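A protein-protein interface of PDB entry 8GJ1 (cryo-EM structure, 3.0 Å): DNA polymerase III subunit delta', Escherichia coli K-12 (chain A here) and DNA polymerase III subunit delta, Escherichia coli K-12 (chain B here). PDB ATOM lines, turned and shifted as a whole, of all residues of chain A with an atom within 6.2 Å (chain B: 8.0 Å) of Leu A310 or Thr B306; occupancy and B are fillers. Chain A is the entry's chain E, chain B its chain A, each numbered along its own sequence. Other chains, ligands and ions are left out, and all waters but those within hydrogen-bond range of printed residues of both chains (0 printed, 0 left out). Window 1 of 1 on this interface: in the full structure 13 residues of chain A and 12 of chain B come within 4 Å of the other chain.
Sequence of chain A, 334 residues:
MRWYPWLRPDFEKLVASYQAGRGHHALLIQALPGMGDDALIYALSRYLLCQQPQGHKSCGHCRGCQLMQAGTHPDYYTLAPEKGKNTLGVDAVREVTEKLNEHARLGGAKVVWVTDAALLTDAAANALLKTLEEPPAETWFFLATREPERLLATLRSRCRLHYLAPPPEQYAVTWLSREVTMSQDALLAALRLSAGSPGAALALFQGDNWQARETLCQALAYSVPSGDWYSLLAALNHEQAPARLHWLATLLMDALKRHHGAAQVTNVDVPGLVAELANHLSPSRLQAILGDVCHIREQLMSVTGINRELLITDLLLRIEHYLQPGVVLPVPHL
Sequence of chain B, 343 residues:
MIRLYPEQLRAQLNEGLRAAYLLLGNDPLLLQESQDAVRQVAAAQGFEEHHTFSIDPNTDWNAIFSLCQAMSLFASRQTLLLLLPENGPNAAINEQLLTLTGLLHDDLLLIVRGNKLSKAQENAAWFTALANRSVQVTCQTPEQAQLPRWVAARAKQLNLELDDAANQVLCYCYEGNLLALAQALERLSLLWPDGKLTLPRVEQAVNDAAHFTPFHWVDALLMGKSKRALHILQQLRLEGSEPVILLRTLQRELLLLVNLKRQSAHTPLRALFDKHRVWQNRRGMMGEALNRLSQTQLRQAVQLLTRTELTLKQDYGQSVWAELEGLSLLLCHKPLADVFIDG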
ATOM      1  N   ASN A 237      -8.615  19.855  19.807  1.00  0.00           N
ATOM      2  CA  ASN A 237      -8.923  19.621  18.402  1.00  0.00           C
ATOM      3  C   ASN A 237      -8.668  20.883  17.590  1.00  0.00           C
ATOM      4  O   ASN A 237      -9.541  21.750  17.484  1.00  0.00           O
ATOM      5  CB  ASN A 237     -10.374  19.166  18.240  1.00  0.00           C
ATOM      6  CG  ASN A 237     -10.692  18.732  16.825  1.00  0.00           C
ATOM      7  OD1 ASN A 237     -10.566  17.557  16.481  1.00  0.00           O
ATOM      8  ND2 ASN A 237     -11.106  19.681  15.994  1.00  0.00           N
ATOM      9  N   ILE A 306      -3.853  11.610   8.668  1.00  0.00           N
ATOM     10  CA  ILE A 306      -4.508  10.994   9.816  1.00  0.00           C
ATOM     11  C   ILE A 306      -5.517  11.972  10.398  1.00  0.00           C
ATOM     12  O   ILE A 306      -5.252  13.174  10.510  1.00  0.00           O
ATOM     13  CB  ILE A 306      -3.464  10.568  10.865  1.00  0.00           C
ATOM     14  CG1 ILE A 306      -4.108   9.711  11.960  1.00  0.00           C
ATOM     15  CG2 ILE A 306      -2.798  11.788  11.488  1.00  0.00           C
ATOM     16  CD1 ILE A 306      -4.570   8.350  11.485  1.00  0.00           C
ATOM     17  N   ASN A 307      -6.687  11.456  10.772  1.00  0.00           N
ATOM     18  CA  ASN A 307      -7.741  12.284  11.345  1.00  0.00           C
ATOM     19  C   ASN A 307      -7.422  12.563  12.810  1.00  0.00           C
ATOM     20  O   ASN A 307      -7.345  11.634  13.622  1.00  0.00           O
ATOM     21  CB  ASN A 307      -9.093  11.592  11.207  1.00  0.00           C
ATOM     22  CG  ASN A 307     -10.248  12.481  11.614  1.00  0.00           C
ATOM     23  OD1 ASN A 307     -10.658  12.492  12.775  1.00  0.00           O
ATOM     24  ND2 ASN A 307     -10.780  13.235  10.660  1.00  0.00           N
ATOM     25  N   ARG A 308      -7.236  13.840  13.148  1.00  0.00           N
ATOM     26  CA  ARG A 308      -6.810  14.191  14.499  1.00  0.00           C
ATOM     27  C   ARG A 308      -7.924  13.993  15.520  1.00  0.00           C
ATOM     28  O   ARG A 308      -7.647  13.642  16.673  1.00  0.00           O
ATOM     29  CB  ARG A 308      -6.315  15.638  14.535  1.00  0.00           C
ATOM     30  CG  ARG A 308      -7.361  16.677  14.159  1.00  0.00           C
ATOM     31  CD  ARG A 308      -6.843  18.087  14.384  1.00  0.00           C
ATOM     32  NE  ARG A 308      -5.716  18.405  13.515  1.00  0.00           N
ATOM     33  CZ  ARG A 308      -5.821  18.910  12.292  1.00  0.00           C
ATOM     34  NH1 ARG A 308      -6.999  19.163  11.744  1.00  0.00           N
ATOM     35  NH2 ARG A 308      -4.715  19.164  11.599  1.00  0.00           N
ATOM     36  N   GLU A 309      -9.178  14.219  15.127  1.00  0.00           N
ATOM     37  CA  GLU A 309     -10.276  14.161  16.087  1.00  0.00           C
ATOM     38  C   GLU A 309     -10.401  12.770  16.698  1.00  0.00           C
ATOM     39  O   GLU A 309     -10.485  12.621  17.922  1.00  0.00           O
ATOM     40  CB  GLU A 309     -11.582  14.572  15.408  1.00  0.00           C
ATOM     41  CG  GLU A 309     -12.769  14.673  16.352  1.00  0.00           C
ATOM     42  CD  GLU A 309     -14.027  15.145  15.653  1.00  0.00           C
ATOM     43  OE1 GLU A 309     -13.984  15.352  14.422  1.00  0.00           O
ATOM     44  OE2 GLU A 309     -15.061  15.311  16.334  1.00  0.00           O
ATOM     45  N   LEU A 310     -10.413  11.736  15.854  1.00  0.00           N
ATOM     46  CA  LEU A 310     -10.540  10.373  16.359  1.00  0.00           C
ATOM     47  C   LEU A 310      -9.355  10.001  17.238  1.00  0.00           C
ATOM     48  O   LEU A 310      -9.523   9.376  18.294  1.00  0.00           O
ATOM     49  CB  LEU A 310     -10.669   9.395  15.191  1.00  0.00           C
ATOM     50  CG  LEU A 310     -10.726   7.907  15.541  1.00  0.00           C
ATOM     51  CD1 LEU A 310     -11.892   7.611  16.469  1.00  0.00           C
ATOM     52  CD2 LEU A 310     -10.825   7.072  14.278  1.00  0.00           C
ATOM     53  N   LEU A 311      -8.146  10.373  16.817  1.00  0.00           N
ATOM     54  CA  LEU A 311      -6.956  10.039  17.590  1.00  0.00           C
ATOM     55  C   LEU A 311      -7.007  10.682  18.969  1.00  0.00           C
ATOM     56  O   LEU A 311      -6.730  10.031  19.984  1.00  0.00           O
ATOM     57  CB  LEU A 311      -5.704  10.484  16.832  1.00  0.00           C
ATOM     58  CG  LEU A 311      -4.484   9.569  16.925  1.00  0.00           C
ATOM     59  CD1 LEU A 311      -4.724   8.270  16.172  1.00  0.00           C
ATOM     60  CD2 LEU A 311      -3.251  10.278  16.389  1.00  0.00           C
ATOM     61  N   ILE A 312      -7.381  11.962  19.028  1.00  0.00           N
ATOM     62  CA  ILE A 312      -7.425  12.659  20.308  1.00  0.00           C
ATOM     63  C   ILE A 312      -8.538  12.098  21.185  1.00  0.00           C
ATOM     64  O   ILE A 312      -8.382  11.980  22.406  1.00  0.00           O
ATOM     65  CB  ILE A 312      -7.584  14.173  20.086  1.00  0.00           C
ATOM     66  CG1 ILE A 312      -6.356  14.731  19.362  1.00  0.00           C
ATOM     67  CG2 ILE A 312      -7.785  14.884  21.421  1.00  0.00           C
ATOM     68  CD1 ILE A 312      -6.523  16.151  18.864  1.00  0.00           C
ATOM     69  N   THR A 313      -9.679  11.751  20.584  1.00  0.00           N
ATOM     70  CA  THR A 313     -10.765  11.168  21.365  1.00  0.00           C
ATOM     71  C   THR A 313     -10.338   9.843  21.981  1.00  0.00           C
ATOM     72  O   THR A 313     -10.585   9.584  23.165  1.00  0.00           O
ATOM     73  CB  THR A 313     -12.000  10.977  20.483  1.00  0.00           C
ATOM     74  OG1 THR A 313     -12.394  12.237  19.926  1.00  0.00           O
ATOM     75  CG2 THR A 313     -13.153  10.404  21.293  1.00  0.00           C
ATOM     76  N   ASP A 314      -9.683   8.990  21.190  1.00  0.00           N
ATOM     77  CA  ASP A 314      -9.201   7.720  21.721  1.00  0.00           C
ATOM     78  C   ASP A 314      -8.167   7.947  22.815  1.00  0.00           C
ATOM     79  O   ASP A 314      -8.169   7.250  23.839  1.00  0.00           O
ATOM     80  CB  ASP A 314      -8.615   6.868  20.598  1.00  0.00           C
ATOM     81  CG  ASP A 314      -8.090   5.536  21.092  1.00  0.00           C
ATOM     82  OD1 ASP A 314      -8.907   4.705  21.541  1.00  0.00           O
ATOM     83  OD2 ASP A 314      -6.862   5.320  21.034  1.00  0.00           O
ATOM     84  N   LEU A 315      -7.272   8.916  22.616  1.00  0.00           N
ATOM     85  CA  LEU A 315      -6.282   9.233  23.639  1.00  0.00           C
ATOM     86  C   LEU A 315      -6.955   9.615  24.949  1.00  0.00           C
ATOM     87  O   LEU A 315      -6.609   9.092  26.014  1.00  0.00           O
ATOM     88  CB  LEU A 315      -5.373  10.362  23.151  1.00  0.00           C
ATOM     89  CG  LEU A 315      -4.467  11.021  24.193  1.00  0.00           C
ATOM     90  CD1 LEU A 315      -3.593   9.988  24.883  1.00  0.00           C
ATOM     91  CD2 LEU A 315      -3.615  12.101  23.547  1.00  0.00           C
ATOM     92  N   ARG A 318      -8.599   6.668  26.669  1.00  0.00           N
ATOM     93  CA  ARG A 318      -7.612   5.820  27.332  1.00  0.00           C
ATOM     94  C   ARG A 318      -7.097   6.469  28.610  1.00  0.00           C
ATOM     95  O   ARG A 318      -6.889   5.785  29.620  1.00  0.00           O
ATOM     96  CB  ARG A 318      -6.451   5.514  26.387  1.00  0.00           C
ATOM     97  CG  ARG A 318      -6.791   4.532  25.282  1.00  0.00           C
ATOM     98  CD  ARG A 318      -5.561   3.759  24.839  1.00  0.00           C
ATOM     99  NE  ARG A 318      -4.437   4.641  24.550  1.00  0.00           N
ATOM    100  CZ  ARG A 318      -4.238   5.259  23.392  1.00  0.00           C
ATOM    101  NH1 ARG A 318      -5.079   5.123  22.379  1.00  0.00           N
ATOM    102  NH2 ARG A 318      -3.169   6.035  23.247  1.00  0.00           N
ATOM    103  N   LEU B 247     -15.026   4.088   6.888  1.00  0.00           N
ATOM    104  CA  LEU B 247     -14.519   4.514   8.187  1.00  0.00           C
ATOM    105  C   LEU B 247     -14.994   5.920   8.526  1.00  0.00           C
ATOM    106  O   LEU B 247     -15.435   6.179   9.651  1.00  0.00           O
ATOM    107  CB  LEU B 247     -12.992   4.449   8.202  1.00  0.00           C
ATOM    108  CG  LEU B 247     -12.358   3.074   7.983  1.00  0.00           C
ATOM    109  CD1 LEU B 247     -10.849   3.202   7.863  1.00  0.00           C
ATOM    110  CD2 LEU B 247     -12.721   2.120   9.105  1.00  0.00           C
ATOM    111  N   ARG B 248     -14.919   6.840   7.563  1.00  0.00           N
ATOM    112  CA  ARG B 248     -15.338   8.212   7.832  1.00  0.00           C
ATOM    113  C   ARG B 248     -16.841   8.298   8.068  1.00  0.00           C
ATOM    114  O   ARG B 248     -17.294   9.061   8.928  1.00  0.00           O
ATOM    115  CB  ARG B 248     -14.917   9.126   6.684  1.00  0.00           C
ATOM    116  CG  ARG B 248     -13.422   9.393   6.632  1.00  0.00           C
ATOM    117  CD  ARG B 248     -12.966  10.300   7.769  1.00  0.00           C
ATOM    118  NE  ARG B 248     -11.572  10.061   8.123  1.00  0.00           N
ATOM    119  CZ  ARG B 248     -11.151   9.051   8.873  1.00  0.00           C
ATOM    120  NH1 ARG B 248     -11.991   8.156   9.366  1.00  0.00           N
ATOM    121  NH2 ARG B 248      -9.852   8.933   9.131  1.00  0.00           N
ATOM    122  N   GLN B 251     -17.426   7.069  11.557  1.00  0.00           N
ATOM    123  CA  GLN B 251     -16.797   7.856  12.613  1.00  0.00           C
ATOM    124  C   GLN B 251     -17.765   8.872  13.202  1.00  0.00           C
ATOM    125  O   GLN B 251     -17.842   9.033  14.425  1.00  0.00           O
ATOM    126  CB  GLN B 251     -15.553   8.556  12.063  1.00  0.00           C
ATOM    127  CG  GLN B 251     -14.846   9.461  13.060  1.00  0.00           C
ATOM    128  CD  GLN B 251     -13.595  10.091  12.487  1.00  0.00           C
ATOM    129  OE1 GLN B 251     -13.080   9.652  11.459  1.00  0.00           O
ATOM    130  NE2 GLN B 251     -13.100  11.131  13.147  1.00  0.00           N
ATOM    131  N   LEU B 254     -20.398   7.140  15.379  1.00  0.00           N
ATOM    132  CA  LEU B 254     -19.820   6.591  16.602  1.00  0.00           C
ATOM    133  C   LEU B 254     -19.488   7.696  17.596  1.00  0.00           C
ATOM    134  O   LEU B 254     -19.761   7.566  18.797  1.00  0.00           O
ATOM    135  CB  LEU B 254     -18.574   5.772  16.268  1.00  0.00           C
ATOM    136  CG  LEU B 254     -17.922   5.020  17.429  1.00  0.00           C
ATOM    137  CD1 LEU B 254     -18.893   4.035  18.058  1.00  0.00           C
ATOM    138  CD2 LEU B 254     -16.670   4.304  16.955  1.00  0.00           C
ATOM    139  N   LEU B 255     -18.899   8.795  17.118  1.00  0.00           N
ATOM    140  CA  LEU B 255     -18.594   9.912  18.004  1.00  0.00           C
ATOM    141  C   LEU B 255     -19.864  10.522  18.579  1.00  0.00           C
ATOM    142  O   LEU B 255     -19.908  10.886  19.761  1.00  0.00           O
ATOM    143  CB  LEU B 255     -17.781  10.970  17.255  1.00  0.00           C
ATOM    144  CG  LEU B 255     -16.256  10.850  17.344  1.00  0.00           C
ATOM    145  CD1 LEU B 255     -15.770  11.237  18.731  1.00  0.00           C
ATOM    146  CD2 LEU B 255     -15.784   9.447  16.990  1.00  0.00           C
ATOM    147  N   ARG B 299     -16.174   2.378  23.711  1.00  0.00           N
ATOM    148  CA  ARG B 299     -14.767   2.701  23.910  1.00  0.00           C
ATOM    149  C   ARG B 299     -13.854   1.674  23.261  1.00  0.00           C
ATOM    150  O   ARG B 299     -12.850   2.043  22.647  1.00  0.00           O
ATOM    151  CB  ARG B 299     -14.443   2.792  25.405  1.00  0.00           C
ATOM    152  CG  ARG B 299     -13.121   3.484  25.699  1.00  0.00           C
ATOM    153  CD  ARG B 299     -12.701   3.335  27.154  1.00  0.00           C
ATOM    154  NE  ARG B 299     -12.150   2.013  27.437  1.00  0.00           N
ATOM    155  CZ  ARG B 299     -12.834   0.988  27.928  1.00  0.00           C
ATOM    156  NH1 ARG B 299     -14.123   1.083  28.217  1.00  0.00           N
ATOM    157  NH2 ARG B 299     -12.207  -0.167  28.138  1.00  0.00           N
ATOM    158  N   GLN B 300     -14.189   0.389  23.387  1.00  0.00           N
ATOM    159  CA  GLN B 300     -13.474  -0.635  22.638  1.00  0.00           C
ATOM    160  C   GLN B 300     -13.672  -0.443  21.141  1.00  0.00           C
ATOM    161  O   GLN B 300     -12.747  -0.657  20.350  1.00  0.00           O
ATOM    162  CB  GLN B 300     -13.945  -2.024  23.066  1.00  0.00           C
ATOM    163  CG  GLN B 300     -13.750  -2.318  24.545  1.00  0.00           C
ATOM    164  CD  GLN B 300     -14.369  -3.637  24.969  1.00  0.00           C
ATOM    165  OE1 GLN B 300     -15.001  -3.727  26.020  1.00  0.00           O
ATOM    166  NE2 GLN B 300     -14.184  -4.671  24.155  1.00  0.00           N
ATOM    167  N   ALA B 301     -14.879  -0.043  20.734  1.00  0.00           N
ATOM    168  CA  ALA B 301     -15.134   0.211  19.320  1.00  0.00           C
ATOM    169  C   ALA B 301     -14.265   1.346  18.800  1.00  0.00           C
ATOM    170  O   ALA B 301     -13.709   1.258  17.701  1.00  0.00           O
ATOM    171  CB  ALA B 301     -16.613   0.527  19.105  1.00  0.00           C
ATOM    172  N   VAL B 302     -14.135   2.424  19.576  1.00  0.00           N
ATOM    173  CA  VAL B 302     -13.291   3.540  19.158  1.00  0.00           C
ATOM    174  C   VAL B 302     -11.838   3.098  19.056  1.00  0.00           C
ATOM    175  O   VAL B 302     -11.123   3.473  18.118  1.00  0.00           O
ATOM    176  CB  VAL B 302     -13.454   4.726  20.128  1.00  0.00           C
ATOM    177  CG1 VAL B 302     -12.423   5.803  19.831  1.00  0.00           C
ATOM    178  CG2 VAL B 302     -14.858   5.298  20.031  1.00  0.00           C
ATOM    179  N   GLN B 303     -11.372   2.309  20.025  1.00  0.00           N
ATOM    180  CA  GLN B 303      -9.998   1.822  19.984  1.00  0.00           C
ATOM    181  C   GLN B 303      -9.756   0.964  18.749  1.00  0.00           C
ATOM    182  O   GLN B 303      -8.734   1.114  18.067  1.00  0.00           O
ATOM    183  CB  GLN B 303      -9.689   1.033  21.256  1.00  0.00           C
ATOM    184  CG  GLN B 303      -8.281   0.462  21.315  1.00  0.00           C
ATOM    185  CD  GLN B 303      -7.939  -0.131  22.671  1.00  0.00           C
ATOM    186  OE1 GLN B 303      -6.814   0.006  23.151  1.00  0.00           O
ATOM    187  NE2 GLN B 303      -8.907  -0.797  23.293  1.00  0.00           N
ATOM    188  N   LEU B 304     -10.685   0.057  18.443  1.00  0.00           N
ATOM    189  CA  LEU B 304     -10.529  -0.788  17.264  1.00  0.00           C
ATOM    190  C   LEU B 304     -10.567   0.040  15.987  1.00  0.00           C
ATOM    191  O   LEU B 304      -9.812  -0.228  15.045  1.00  0.00           O
ATOM    192  CB  LEU B 304     -11.615  -1.864  17.242  1.00  0.00           C
ATOM    193  CG  LEU B 304     -11.585  -2.836  16.059  1.00  0.00           C
ATOM    194  CD1 LEU B 304     -10.224  -3.499  15.930  1.00  0.00           C
ATOM    195  CD2 LEU B 304     -12.672  -3.887  16.203  1.00  0.00           C
ATOM    196  N   LEU B 305     -11.439   1.048  15.933  1.00  0.00           N
ATOM    197  CA  LEU B 305     -11.498   1.913  14.760  1.00  0.00           C
ATOM    198  C   LEU B 305     -10.186   2.660  14.566  1.00  0.00           C
ATOM    199  O   LEU B 305      -9.681   2.762  13.442  1.00  0.00           O
ATOM    200  CB  LEU B 305     -12.661   2.896  14.899  1.00  0.00           C
ATOM    201  CG  LEU B 305     -12.913   3.842  13.723  1.00  0.00           C
ATOM    202  CD1 LEU B 305     -13.347   3.066  12.495  1.00  0.00           C
ATOM    203  CD2 LEU B 305     -13.953   4.885  14.094  1.00  0.00           C
ATOM    204  N   THR B 306      -9.618   3.190  15.651  1.00  0.00           N
ATOM    205  CA  THR B 306      -8.346   3.896  15.548  1.00  0.00           C
ATOM    206  C   THR B 306      -7.231   2.955  15.111  1.00  0.00           C
ATOM    207  O   THR B 306      -6.384   3.321  14.287  1.00  0.00           O
ATOM    208  CB  THR B 306      -7.999   4.552  16.883  1.00  0.00           C
ATOM    209  OG1 THR B 306      -9.034   5.472  17.249  1.00  0.00           O
ATOM    210  CG2 THR B 306      -6.676   5.295  16.787  1.00  0.00           C
ATOM    211  N   ARG B 307      -7.210   1.738  15.660  1.00  0.00           N
ATOM    212  CA  ARG B 307      -6.187   0.776  15.265  1.00  0.00           C
ATOM    213  C   ARG B 307      -6.312   0.424  13.789  1.00  0.00           C
ATOM    214  O   ARG B 307      -5.305   0.335  13.077  1.00  0.00           O
ATOM    215  CB  ARG B 307      -6.289  -0.481  16.128  1.00  0.00           C
ATOM    216  CG  ARG B 307      -5.126  -1.442  15.953  1.00  0.00           C
ATOM    217  CD  ARG B 307      -5.196  -2.592  16.944  1.00  0.00           C
ATOM    218  NE  ARG B 307      -6.328  -3.474  16.687  1.00  0.00           N
ATOM    219  CZ  ARG B 307      -6.322  -4.476  15.817  1.00  0.00           C
ATOM    220  NH1 ARG B 307      -5.258  -4.749  15.080  1.00  0.00           N
ATOM    221  NH2 ARG B 307      -7.413  -5.223  15.683  1.00  0.00           N
ATOM    222  N   THR B 308      -7.541   0.222  13.310  1.00  0.00           N
ATOM    223  CA  THR B 308      -7.745  -0.075  11.896  1.00  0.00           C
ATOM    224  C   THR B 308      -7.315   1.095  11.022  1.00  0.00           C
ATOM    225  O   THR B 308      -6.700   0.898   9.966  1.00  0.00           O
ATOM    226  CB  THR B 308      -9.211  -0.422  11.638  1.00  0.00           C
ATOM    227  OG1 THR B 308      -9.582  -1.561  12.424  1.00  0.00           O
ATOM    228  CG2 THR B 308      -9.439  -0.727  10.166  1.00  0.00           C
ATOM    229  N   GLU B 309      -7.634   2.322  11.438  1.00  0.00           N
ATOM    230  CA  GLU B 309      -7.216   3.488  10.671  1.00  0.00           C
ATOM    231  C   GLU B 309      -5.699   3.567  10.585  1.00  0.00           C
ATOM    232  O   GLU B 309      -5.142   3.833   9.513  1.00  0.00           O
ATOM    233  CB  GLU B 309      -7.780   4.761  11.301  1.00  0.00           C
ATOM    234  CG  GLU B 309      -7.525   6.024  10.489  1.00  0.00           C
ATOM    235  CD  GLU B 309      -7.864   7.288  11.252  1.00  0.00           C
ATOM    236  OE1 GLU B 309      -7.915   7.239  12.498  1.00  0.00           O
ATOM    237  OE2 GLU B 309      -8.079   8.335  10.604  1.00  0.00           O
ATOM    238  N   LEU B 310      -5.013   3.349  11.709  1.00  0.00           N
ATOM    239  CA  LEU B 310      -3.555   3.393  11.697  1.00  0.00           C
ATOM    240  C   LEU B 310      -2.980   2.291  10.819  1.00  0.00           C
ATOM    241  O   LEU B 310      -2.031   2.523  10.063  1.00  0.00           O
ATOM    242  CB  LEU B 310      -3.011   3.281  13.121  1.00  0.00           C
ATOM    243  CG  LEU B 310      -3.202   4.510  14.014  1.00  0.00           C
ATOM    244  CD1 LEU B 310      -2.768   4.199  15.437  1.00  0.00           C
ATOM    245  CD2 LEU B 310      -2.433   5.704  13.469  1.00  0.00           C
ATOM    246  N   THR B 311      -3.545   1.085  10.897  1.00  0.00           N
ATOM    247  CA  THR B 311      -3.060  -0.006  10.058  1.00  0.00           C
ATOM    248  C   THR B 311      -3.233   0.321   8.581  1.00  0.00           C
ATOM    249  O   THR B 311      -2.336   0.067   7.771  1.00  0.00           O
ATOM    250  CB  THR B 311      -3.793  -1.302  10.405  1.00  0.00           C
ATOM    251  OG1 THR B 311      -3.558  -1.635  11.779  1.00  0.00           O
ATOM    252  CG2 THR B 311      -3.315  -2.444   9.519  1.00  0.00           C
ATOM    253  N   LEU B 312      -4.383   0.887   8.213  1.00  0.00           N
ATOM    254  CA  LEU B 312      -4.632   1.214   6.813  1.00  0.00           C
ATOM    255  C   LEU B 312      -3.707   2.325   6.330  1.00  0.00           C
ATOM    256  O   LEU B 312      -3.132   2.236   5.238  1.00  0.00           O
ATOM    257  CB  LEU B 312      -6.096   1.617   6.627  1.00  0.00           C
ATOM    258  CG  LEU B 312      -6.477   2.255   5.287  1.00  0.00           C
ATOM    259  CD1 LEU B 312      -6.097   1.354   4.122  1.00  0.00           C
ATOM    260  CD2 LEU B 312      -7.963   2.569   5.258  1.00  0.00           C
ATOM    261  N   LYS B 313      -3.546   3.377   7.129  1.00  0.00           N
ATOM    262  CA  LYS B 313      -2.892   4.594   6.666  1.00  0.00           C
ATOM    263  C   LYS B 313      -1.395   4.630   6.945  1.00  0.00           C
ATOM    264  O   LYS B 313      -0.722   5.554   6.474  1.00  0.00           O
ATOM    265  CB  LYS B 313      -3.561   5.809   7.316  1.00  0.00           C
ATOM    266  CG  LYS B 313      -3.360   7.112   6.561  1.00  0.00           C
ATOM    267  CD  LYS B 313      -4.301   8.203   7.057  1.00  0.00           C
ATOM    268  CE  LYS B 313      -5.734   7.970   6.594  1.00  0.00           C
ATOM    269  NZ  LYS B 313      -6.641   9.077   6.999  1.00  0.00           N
ATOM    270  N   GLU B 323     -10.934  -6.613   9.971  1.00  0.00           N
ATOM    271  CA  GLU B 323     -11.139  -5.751  11.129  1.00  0.00           C
ATOM    272  C   GLU B 323     -12.493  -5.057  11.066  1.00  0.00           C
ATOM    273  O   GLU B 323     -13.149  -4.869  12.095  1.00  0.00           O
ATOM    274  CB  GLU B 323     -10.009  -4.728  11.224  1.00  0.00           C
ATOM    275  CG  GLU B 323      -8.643  -5.352  11.448  1.00  0.00           C
ATOM    276  CD  GLU B 323      -7.538  -4.320  11.524  1.00  0.00           C
ATOM    277  OE1 GLU B 323      -7.824  -3.129  11.285  1.00  0.00           O
ATOM    278  OE2 GLU B 323      -6.386  -4.698  11.822  1.00  0.00           O
ATOM    279  N   LEU B 327     -15.361  -5.335  13.880  1.00  0.00           N
ATOM    280  CA  LEU B 327     -15.998  -4.168  14.483  1.00  0.00           C
ATOM    281  C   LEU B 327     -17.507  -4.201  14.277  1.00  0.00           C
ATOM    282  O   LEU B 327     -18.269  -3.800  15.162  1.00  0.00           O
ATOM    283  CB  LEU B 327     -15.392  -2.890  13.899  1.00  0.00           C
ATOM    284  CG  LEU B 327     -15.785  -1.521  14.478  1.00  0.00           C
ATOM    285  CD1 LEU B 327     -17.054  -0.979  13.836  1.00  0.00           C
ATOM    286  CD2 LEU B 327     -15.937  -1.559  15.995  1.00  0.00           C
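Among the printed residues, pairs that only touch across the chains: Leu A310 with Glu B309 (3.4 Å), Leu A310 with Thr B306 (3.4 Å), Asp A314 with Gln B303 (3.5 Å), Asn A307 with Arg B248 (3.5 Å), Ile A306 with Glu B309 (3.5 Å), Leu A311 with Thr B306 (3.6 Å), Leu A310 with Gln B251 (3.6 Å), Asp A314 with Thr B306 (3.7 Å), Thr A313 with Leu B255 (3.7 Å), Ile A306 with Lys B313 (3.8 Å), Leu A310 with Leu B305 (3.8 Å), Leu A310 with Val B302 (3.9 Å) and Ile A306 with Leu B310 (3.9 Å).
The side-chain amide oxygen (OE1) of Gln B251 lies within hydrogen-bond range of the guanidinium group (NH1) of Arg B248.
OE2 of Glu B309 lies within salt-bridge range of NZ of Lys B313 (3.95 Å).
The side-chain amide oxygen (OD1) of Asn A307 sits at hydrogen-bond distance from the backbone NH (N) of Glu A309 (3.3 Å).
The side-chain amide oxygen (OD1) of Asn A307 lies within hydrogen-bond range of the backbone NH (N) of Leu A310, at 3.2 Å.
O of Glu A309 is in hydrogen-bond range of OG1 of Thr A313 (2.8 Å).
OD1 of Asp A314 is in salt-bridge range of NH1 of Arg A318 (3.9 Å).
NE2 of Gln B251 sits at hydrogen-bond distance from OD1 of Asn A307 (2.8 Å).
OE2 of Glu B309 sits at hydrogen-bond distance from N of Asn A307 (3.4 Å).
Of the printed residues of chain B, Ile A306 touches Glu B309 (3.5 Å), Leu B310 (3.9 Å) and Lys B313 (3.8 Å).
Leu A310 touches just these residues of chain B: Gln B251, Val B302, Leu B305, Thr B306 and Glu B309.
Of the printed residues of chain B, Thr A313 touches Leu B255.
Arg B299 touches none of the printed residues of chain A.
Gln B300 touches none of the printed residues of chain A.
Printed residues of chain A within 4 Å of Gln B303: Asp A314.
Printed residues of chain A within 4 Å of Thr B306: Leu A310 (3.4 Å), Leu A311 (3.6 Å) and Asp A314 (3.7 Å).
Printed residues of chain A within 4 Å of Leu B310: Ile A306 (3.9 Å).
Printed residues of chain A within 4 Å of Lys B313: Ile A306.
The nearest residue of chain B that does not touch Leu A310 is Leu B255 (4.3 Å).
Hydrophobic or aromatic side chains of chain A that line the printed part of chain B: Ile A306, Leu A310 and Leu A311.
Among the printed residues, 15 pairs touch across the chains.
Among the printed residues, no Asp or Glu carboxylate lies within 4 Å of a Lys or Arg side-chain nitrogen of the other chain.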
